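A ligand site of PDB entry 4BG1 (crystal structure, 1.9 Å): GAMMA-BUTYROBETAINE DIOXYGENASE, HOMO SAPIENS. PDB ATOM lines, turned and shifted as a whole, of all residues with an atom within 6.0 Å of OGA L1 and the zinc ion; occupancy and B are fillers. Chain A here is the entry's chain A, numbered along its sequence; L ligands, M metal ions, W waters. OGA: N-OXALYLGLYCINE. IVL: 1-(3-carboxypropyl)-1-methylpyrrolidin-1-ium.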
ATOM      1  N   TRP A 181      22.612 -28.443 -13.792  1.00  0.00           N
ATOM      2  CA  TRP A 181      21.367 -27.682 -13.887  1.00  0.00           C
ATOM      3  C   TRP A 181      21.612 -26.204 -13.630  1.00  0.00           C
ATOM      4  O   TRP A 181      22.574 -25.826 -12.929  1.00  0.00           O
ATOM      5  CB  TRP A 181      20.275 -28.240 -12.948  1.00  0.00           C
ATOM      6  CG  TRP A 181      20.797 -28.964 -11.772  1.00  0.00           C
ATOM      7  CD1 TRP A 181      21.016 -30.303 -11.672  1.00  0.00           C
ATOM      8  CD2 TRP A 181      21.165 -28.400 -10.501  1.00  0.00           C
ATOM      9  NE1 TRP A 181      21.505 -30.611 -10.418  1.00  0.00           N
ATOM     10  CE2 TRP A 181      21.630 -29.467  -9.694  1.00  0.00           C
ATOM     11  CE3 TRP A 181      21.171 -27.105  -9.985  1.00  0.00           C
ATOM     12  CZ2 TRP A 181      22.071 -29.274  -8.386  1.00  0.00           C
ATOM     13  CZ3 TRP A 181      21.608 -26.921  -8.687  1.00  0.00           C
ATOM     14  CH2 TRP A 181      22.049 -28.010  -7.900  1.00  0.00           C
ATOM     15  N   VAL A 183      20.497 -22.725 -12.067  1.00  0.00           N
ATOM     16  CA  VAL A 183      19.660 -22.022 -11.106  1.00  0.00           C
ATOM     17  C   VAL A 183      19.493 -20.578 -11.557  1.00  0.00           C
ATOM     18  O   VAL A 183      20.419 -19.786 -11.448  1.00  0.00           O
ATOM     19  CB  VAL A 183      20.220 -22.098  -9.662  1.00  0.00           C
ATOM     20  CG1 VAL A 183      19.232 -21.528  -8.666  1.00  0.00           C
ATOM     21  CG2 VAL A 183      20.592 -23.520  -9.301  1.00  0.00           C
ATOM     22  N   ASN A 191      10.353 -25.846 -10.444  1.00  0.00           N
ATOM     23  CA  ASN A 191      10.924 -25.981  -9.094  1.00  0.00           C
ATOM     24  C   ASN A 191      11.004 -24.590  -8.479  1.00  0.00           C
ATOM     25  O   ASN A 191      11.350 -23.624  -9.172  1.00  0.00           O
ATOM     26  CB  ASN A 191      12.322 -26.623  -9.198  1.00  0.00           C
ATOM     27  CG  ASN A 191      12.848 -27.133  -7.853  1.00  0.00           C
ATOM     28  OD1 ASN A 191      13.268 -26.358  -6.995  1.00  0.00           O
ATOM     29  ND2 ASN A 191      12.847 -28.440  -7.688  1.00  0.00           N
ATOM     30  N   ALA A 193      13.234 -23.330  -6.760  1.00  0.00           N
ATOM     31  CA  ALA A 193      14.596 -22.802  -6.881  1.00  0.00           C
ATOM     32  C   ALA A 193      14.769 -21.942  -8.123  1.00  0.00           C
ATOM     33  O   ALA A 193      15.603 -21.021  -8.153  1.00  0.00           O
ATOM     34  CB  ALA A 193      15.598 -23.958  -6.883  1.00  0.00           C
ATOM     35  N   TYR A 194      13.959 -22.229  -9.132  1.00  0.00           N
ATOM     36  CA  TYR A 194      14.043 -21.536 -10.410  1.00  0.00           C
ATOM     37  C   TYR A 194      13.110 -20.303 -10.453  1.00  0.00           C
ATOM     38  O   TYR A 194      12.515 -19.987 -11.475  1.00  0.00           O
ATOM     39  CB  TYR A 194      13.733 -22.502 -11.565  1.00  0.00           C
ATOM     40  CG  TYR A 194      14.673 -23.688 -11.714  1.00  0.00           C
ATOM     41  CD1 TYR A 194      16.006 -23.628 -11.294  1.00  0.00           C
ATOM     42  CD2 TYR A 194      14.249 -24.849 -12.360  1.00  0.00           C
ATOM     43  CE1 TYR A 194      16.854 -24.706 -11.450  1.00  0.00           C
ATOM     44  CE2 TYR A 194      15.100 -25.937 -12.518  1.00  0.00           C
ATOM     45  CZ  TYR A 194      16.405 -25.857 -12.072  1.00  0.00           C
ATOM     46  OH  TYR A 194      17.248 -26.903 -12.235  1.00  0.00           O
ATOM     47  N   LEU A 199      14.654 -19.128  -0.511  1.00  0.00           N
ATOM     48  CA  LEU A 199      14.618 -20.551  -0.186  1.00  0.00           C
ATOM     49  C   LEU A 199      15.037 -20.647   1.262  1.00  0.00           C
ATOM     50  O   LEU A 199      16.163 -20.230   1.630  1.00  0.00           O
ATOM     51  CB  LEU A 199      15.565 -21.377  -1.064  1.00  0.00           C
ATOM     52  CG  LEU A 199      15.351 -21.264  -2.588  1.00  0.00           C
ATOM     53  CD1 LEU A 199      16.422 -22.030  -3.344  1.00  0.00           C
ATOM     54  CD2 LEU A 199      13.979 -21.798  -2.942  1.00  0.00           C
ATOM     55  N   HIS A 202      16.829 -26.032   3.515  1.00  0.00           N
ATOM     56  CA  HIS A 202      16.436 -27.345   3.008  1.00  0.00           C
ATOM     57  C   HIS A 202      17.672 -28.170   2.651  1.00  0.00           C
ATOM     58  O   HIS A 202      18.768 -27.621   2.475  1.00  0.00           O
ATOM     59  CB  HIS A 202      15.580 -27.196   1.754  1.00  0.00           C
ATOM     60  CG  HIS A 202      16.308 -26.569   0.607  1.00  0.00           C
ATOM     61  ND1 HIS A 202      16.603 -25.232   0.569  1.00  0.00           N
ATOM     62  CD2 HIS A 202      16.824 -27.098  -0.528  1.00  0.00           C
ATOM     63  CE1 HIS A 202      17.250 -24.950  -0.562  1.00  0.00           C
ATOM     64  NE2 HIS A 202      17.384 -26.074  -1.235  1.00  0.00           N
ATOM     65  N   THR A 203      17.479 -29.481   2.531  1.00  0.00           N
ATOM     66  CA  THR A 203      18.378 -30.402   1.840  1.00  0.00           C
ATOM     67  C   THR A 203      17.817 -30.580   0.452  1.00  0.00           C
ATOM     68  O   THR A 203      16.622 -30.481   0.279  1.00  0.00           O
ATOM     69  CB  THR A 203      18.474 -31.769   2.532  1.00  0.00           C
ATOM     70  OG1 THR A 203      17.174 -32.385   2.634  1.00  0.00           O
ATOM     71  CG2 THR A 203      19.049 -31.608   3.961  1.00  0.00           C
ATOM     72  N   ASP A 204      18.669 -30.846  -0.528  1.00  0.00           N
ATOM     73  CA  ASP A 204      18.178 -31.100  -1.888  1.00  0.00           C
ATOM     74  C   ASP A 204      17.733 -32.535  -2.098  1.00  0.00           C
ATOM     75  O   ASP A 204      18.390 -33.492  -1.686  1.00  0.00           O
ATOM     76  CB  ASP A 204      19.221 -30.775  -2.943  1.00  0.00           C
ATOM     77  CG  ASP A 204      19.197 -29.325  -3.387  1.00  0.00           C
ATOM     78  OD1 ASP A 204      18.707 -28.460  -2.636  1.00  0.00           O
ATOM     79  OD2 ASP A 204      19.663 -29.077  -4.533  1.00  0.00           O
ATOM     80  N   GLN A 215      26.699 -31.727  -2.926  1.00  0.00           N
ATOM     81  CA  GLN A 215      26.183 -30.782  -3.881  1.00  0.00           C
ATOM     82  C   GLN A 215      27.288 -29.763  -4.271  1.00  0.00           C
ATOM     83  O   GLN A 215      28.078 -29.334  -3.440  1.00  0.00           O
ATOM     84  CB  GLN A 215      24.978 -30.037  -3.288  1.00  0.00           C
ATOM     85  CG  GLN A 215      24.343 -29.012  -4.199  1.00  0.00           C
ATOM     86  CD  GLN A 215      22.945 -28.567  -3.743  1.00  0.00           C
ATOM     87  OE1 GLN A 215      22.442 -27.535  -4.167  1.00  0.00           O
ATOM     88  NE2 GLN A 215      22.343 -29.326  -2.864  1.00  0.00           N
ATOM     89  N   LEU A 217      27.703 -26.017  -6.220  1.00  0.00           N
ATOM     90  CA  LEU A 217      27.060 -24.806  -6.766  1.00  0.00           C
ATOM     91  C   LEU A 217      28.097 -23.771  -7.148  1.00  0.00           C
ATOM     92  O   LEU A 217      28.865 -23.307  -6.309  1.00  0.00           O
ATOM     93  CB  LEU A 217      26.118 -24.134  -5.766  1.00  0.00           C
ATOM     94  CG  LEU A 217      24.761 -24.712  -5.424  1.00  0.00           C
ATOM     95  CD1 LEU A 217      24.078 -23.830  -4.377  1.00  0.00           C
ATOM     96  CD2 LEU A 217      23.903 -24.785  -6.674  1.00  0.00           C
ATOM     97  N   GLY A 227      19.883 -12.481  -2.804  1.00  0.00           N
ATOM     98  CA  GLY A 227      20.491 -13.725  -3.264  1.00  0.00           C
ATOM     99  C   GLY A 227      21.690 -14.199  -2.468  1.00  0.00           C
ATOM    100  O   GLY A 227      22.429 -15.060  -2.932  1.00  0.00           O
ATOM    101  N   ASP A 228      21.866 -13.662  -1.254  1.00  0.00           N
ATOM    102  CA  ASP A 228      22.854 -14.199  -0.285  1.00  0.00           C
ATOM    103  C   ASP A 228      22.549 -15.659   0.050  1.00  0.00           C
ATOM    104  O   ASP A 228      21.382 -16.082   0.029  1.00  0.00           O
ATOM    105  CB  ASP A 228      22.837 -13.414   1.047  1.00  0.00           C
ATOM    106  CG  ASP A 228      22.948 -11.913   0.860  1.00  0.00           C
ATOM    107  OD1 ASP A 228      22.031 -11.308   0.288  1.00  0.00           O
ATOM    108  OD2 ASP A 228      23.994 -11.353   1.267  1.00  0.00           O
ATOM    109  N   SER A 229      23.590 -16.409   0.410  1.00  0.00           N
ATOM    110  CA  SER A 229      23.508 -17.807   0.804  1.00  0.00           C
ATOM    111  C   SER A 229      23.510 -17.936   2.302  1.00  0.00           C
ATOM    112  O   SER A 229      24.076 -17.095   3.006  1.00  0.00           O
ATOM    113  CB  SER A 229      24.705 -18.555   0.217  1.00  0.00           C
ATOM    114  OG  SER A 229      24.699 -18.448  -1.184  1.00  0.00           O
ATOM    115  N   MET A 332      27.884 -15.426  -2.535  1.00  0.00           N
ATOM    116  CA  MET A 332      28.722 -15.922  -3.621  1.00  0.00           C
ATOM    117  C   MET A 332      28.974 -14.840  -4.668  1.00  0.00           C
ATOM    118  O   MET A 332      28.076 -14.058  -4.993  1.00  0.00           O
ATOM    119  CB  MET A 332      28.049 -17.130  -4.287  1.00  0.00           C
ATOM    120  CG  MET A 332      27.810 -18.281  -3.337  1.00  0.00           C
ATOM    121  SD  MET A 332      27.402 -19.833  -4.178  1.00  0.00           S
ATOM    122  CE  MET A 332      29.021 -20.285  -4.766  1.00  0.00           C
ATOM    123  N   PHE A 340      29.397 -29.051  -0.805  1.00  0.00           N
ATOM    124  CA  PHE A 340      28.968 -29.320   0.549  1.00  0.00           C
ATOM    125  C   PHE A 340      28.252 -30.653   0.695  1.00  0.00           C
ATOM    126  O   PHE A 340      27.804 -31.255  -0.304  1.00  0.00           O
ATOM    127  CB  PHE A 340      28.165 -28.119   1.115  1.00  0.00           C
ATOM    128  CG  PHE A 340      26.923 -27.770   0.323  1.00  0.00           C
ATOM    129  CD1 PHE A 340      25.710 -28.363   0.630  1.00  0.00           C
ATOM    130  CD2 PHE A 340      26.978 -26.842  -0.688  1.00  0.00           C
ATOM    131  CE1 PHE A 340      24.576 -28.041  -0.084  1.00  0.00           C
ATOM    132  CE2 PHE A 340      25.837 -26.519  -1.409  1.00  0.00           C
ATOM    133  CZ  PHE A 340      24.634 -27.129  -1.113  1.00  0.00           C
ATOM    134  N   HIS A 347      20.749 -25.684   3.496  1.00  0.00           N
ATOM    135  CA  HIS A 347      21.141 -24.473   2.827  1.00  0.00           C
ATOM    136  C   HIS A 347      19.933 -23.712   2.362  1.00  0.00           C
ATOM    137  O   HIS A 347      18.803 -24.265   2.260  1.00  0.00           O
ATOM    138  CB  HIS A 347      22.079 -24.789   1.687  1.00  0.00           C
ATOM    139  CG  HIS A 347      21.469 -25.598   0.581  1.00  0.00           C
ATOM    140  ND1 HIS A 347      21.253 -26.964   0.680  1.00  0.00           N
ATOM    141  CD2 HIS A 347      21.021 -25.244  -0.653  1.00  0.00           C
ATOM    142  CE1 HIS A 347      20.728 -27.406  -0.444  1.00  0.00           C
ATOM    143  NE2 HIS A 347      20.553 -26.382  -1.258  1.00  0.00           N
ATOM    144  N   GLY A 348      20.143 -22.432   2.090  1.00  0.00           N
ATOM    145  CA  GLY A 348      19.061 -21.549   1.666  1.00  0.00           C
ATOM    146  C   GLY A 348      19.600 -20.328   0.947  1.00  0.00           C
ATOM    147  O   GLY A 348      20.799 -20.173   0.752  1.00  0.00           O
ATOM    148  N   ARG A 349      18.687 -19.490   0.504  1.00  0.00           N
ATOM    149  CA  ARG A 349      19.078 -18.261  -0.109  1.00  0.00           C
ATOM    150  C   ARG A 349      18.040 -17.167   0.124  1.00  0.00           C
ATOM    151  O   ARG A 349      16.825 -17.432   0.233  1.00  0.00           O
ATOM    152  CB  ARG A 349      19.310 -18.417  -1.616  1.00  0.00           C
ATOM    153  CG  ARG A 349      18.076 -18.650  -2.416  1.00  0.00           C
ATOM    154  CD  ARG A 349      18.116 -18.052  -3.821  1.00  0.00           C
ATOM    155  NE  ARG A 349      16.775 -18.170  -4.358  1.00  0.00           N
ATOM    156  CZ  ARG A 349      16.387 -18.932  -5.379  1.00  0.00           C
ATOM    157  NH1 ARG A 349      17.253 -19.668  -6.085  1.00  0.00           N
ATOM    158  NH2 ARG A 349      15.100 -18.932  -5.703  1.00  0.00           N
ATOM    159  N   ARG A 360      21.107 -13.325 -12.229  1.00  0.00           N
ATOM    160  CA  ARG A 360      21.658 -14.262 -11.277  1.00  0.00           C
ATOM    161  C   ARG A 360      21.584 -15.653 -11.885  1.00  0.00           C
ATOM    162  O   ARG A 360      20.552 -16.047 -12.404  1.00  0.00           O
ATOM    163  CB  ARG A 360      20.873 -14.227  -9.966  1.00  0.00           C
ATOM    164  CG  ARG A 360      21.543 -15.015  -8.872  1.00  0.00           C
ATOM    165  CD  ARG A 360      20.744 -14.963  -7.601  1.00  0.00           C
ATOM    166  NE  ARG A 360      21.442 -15.542  -6.441  1.00  0.00           N
ATOM    167  CZ  ARG A 360      21.348 -16.812  -6.016  1.00  0.00           C
ATOM    168  NH1 ARG A 360      20.624 -17.724  -6.648  1.00  0.00           N
ATOM    169  NH2 ARG A 360      22.013 -17.183  -4.923  1.00  0.00           N
ATOM    170  N   LEU A 362      23.446 -19.616 -11.172  1.00  0.00           N
ATOM    171  CA  LEU A 362      24.357 -20.608 -10.613  1.00  0.00           C
ATOM    172  C   LEU A 362      24.271 -21.859 -11.472  1.00  0.00           C
ATOM    173  O   LEU A 362      23.191 -22.166 -11.957  1.00  0.00           O
ATOM    174  CB  LEU A 362      23.994 -20.956  -9.175  1.00  0.00           C
ATOM    175  CG  LEU A 362      23.622 -19.864  -8.168  1.00  0.00           C
ATOM    176  CD1 LEU A 362      23.317 -20.523  -6.824  1.00  0.00           C
ATOM    177  CD2 LEU A 362      24.732 -18.848  -7.998  1.00  0.00           C
ATOM    178  N   TYR A 366      25.480 -32.749  -8.538  1.00  0.00           N
ATOM    179  CA  TYR A 366      25.545 -33.614  -7.377  1.00  0.00           C
ATOM    180  C   TYR A 366      26.604 -34.710  -7.587  1.00  0.00           C
ATOM    181  O   TYR A 366      26.926 -35.047  -8.727  1.00  0.00           O
ATOM    182  CB  TYR A 366      24.194 -34.321  -7.153  1.00  0.00           C
ATOM    183  CG  TYR A 366      23.004 -33.411  -6.941  1.00  0.00           C
ATOM    184  CD1 TYR A 366      22.950 -32.558  -5.842  1.00  0.00           C
ATOM    185  CD2 TYR A 366      21.898 -33.449  -7.792  1.00  0.00           C
ATOM    186  CE1 TYR A 366      21.868 -31.722  -5.621  1.00  0.00           C
ATOM    187  CE2 TYR A 366      20.801 -32.612  -7.586  1.00  0.00           C
ATOM    188  CZ  TYR A 366      20.784 -31.764  -6.480  1.00  0.00           C
ATOM    189  OH  TYR A 366      19.717 -30.910  -6.233  1.00  0.00           O
HETATM  190  C1  OGA L   1      18.757 -24.937  -5.074  1.00  0.00           C
HETATM  191  C2  OGA L   1      19.346 -23.973  -4.157  1.00  0.00           C
HETATM  192  C4  OGA L   1      20.591 -21.936  -3.801  1.00  0.00           C
HETATM  193  C5  OGA L   1      20.716 -20.572  -4.465  1.00  0.00           C
HETATM  194  O1  OGA L   1      18.732 -24.655  -6.302  1.00  0.00           O
HETATM  195  O2  OGA L   1      18.327 -26.017  -4.593  1.00  0.00           O
HETATM  196  O2' OGA L   1      19.451 -24.280  -2.975  1.00  0.00           O
HETATM  197  O3  OGA L   1      21.436 -19.729  -3.900  1.00  0.00           O
HETATM  198  N1  OGA L   1      19.795 -22.836  -4.637  1.00  0.00           N
HETATM  199  O4  OGA L   1      20.111 -20.344  -5.524  1.00  0.00           O
HETATM  200  CAF IVL L   2      18.404 -27.710  -8.216  1.00  0.00           C
HETATM  201  CAE IVL L   2      17.611 -26.491  -8.614  1.00  0.00           C
HETATM  202  CAD IVL L   2      16.160 -26.915  -8.704  1.00  0.00           C
HETATM  203  CAA IVL L   2      16.243 -28.405  -8.974  1.00  0.00           C
HETATM  204  CAH IVL L   2      18.062 -30.072  -8.806  1.00  0.00           C
HETATM  205  CAJ IVL L   2      17.270 -28.960  -6.777  1.00  0.00           C
HETATM  206  CAK IVL L   2      16.282 -29.922  -6.259  1.00  0.00           C
HETATM  207  CAL IVL L   2      15.818 -29.306  -4.912  1.00  0.00           C
HETATM  208  CAM IVL L   2      14.661 -30.177  -4.576  1.00  0.00           C
HETATM  209  N3  IVL L   2      17.449 -28.857  -8.223  1.00  0.00           N
HETATM  210  OAB IVL L   2      14.607 -30.833  -3.564  1.00  0.00           O
HETATM  211  OAC IVL L   2      13.721 -30.232  -5.482  1.00  0.00           O
HETATM  212 ZN    ZN M   1      18.913 -26.366  -2.676  1.00  0.00          ZN
HETATM  213  O   HOH W   1      22.683 -20.398  -1.649  1.00  0.00           O
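The guanidinium group (NH2) of Arg 360 is in salt-bridge range of an oxygen (O3) of OGA L1, at 2.8 Å.
The guanidinium group of Arg 349 is in salt-bridge range of an oxygen (O4) of OGA L1, 3.0 Å away.
An oxygen (OAC) of IVL L2 sits at hydrogen-bond distance from the side-chain amide nitrogen of Asn 191 (3.0 Å).
The zinc ion is bound by an oxygen (O2) of OGA L1, the side-chain carboxylate (OD1) of Asp 204, a ring nitrogen (NE2) of His 202, a ring nitrogen (NE2) of His 347 and an oxygen (O2') of OGA L1.
Of the 22 residues printed, 3 come within 4 Å of the zinc ion.
The nearest printed residue that does not touch the zinc ion is Gln 215 (4.01 Å).
The side-chain carboxylate (OD2) of Asp 204 is in hydrogen-bond range of the side-chain amide nitrogen (NE2) of Gln 215, at 3.2 Å.
The side-chain carboxylate (OD2) of Asp 204 lies within hydrogen-bond range of the side-chain hydroxyl (OH) of Tyr 366 (2.5 Å).
The guanidinium group of Arg 360 is in hydrogen-bond range of the backbone carbonyl oxygen of Gly 227 (2.9 Å).
The guanidinium group (NH1) of Arg 349 lies within hydrogen-bond range of the backbone carbonyl oxygen (O) of Ala 193, at 3.0 Å.
O of Arg 349 sits at hydrogen-bond distance from N of Leu 199 (2.9 Å).
The side-chain amide oxygen (OD1) of Asn 191 sits at hydrogen-bond distance from the backbone NH (N) of Ala 193 (3.0 Å).
The backbone carbonyl oxygen (O) of Leu 362 lies within hydrogen-bond range of the backbone NH (N) of Val 183 (2.8 Å).
Water W1 lies within hydrogen-bond range of an oxygen (O3) of OGA L1 (2.7 Å), the side-chain hydroxyl of Ser 229 (2.8 Å) and the backbone carbonyl oxygen of Gly 348 (3.1 Å).
Residues that only touch OGA L1: Val 183, Ala 193, Leu 199 and Leu 362.
Hydrophobic or aromatic side chains that line OGA L1: Val 183, Ala 193, Leu 199, His 202, His 347 and Leu 362.
Nine residues have an atom within 4 Å of OGA L1: Val 183, Ala 193, Leu 199, His 202, Asp 204, His 347, Arg 349, Arg 360 and Leu 362.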
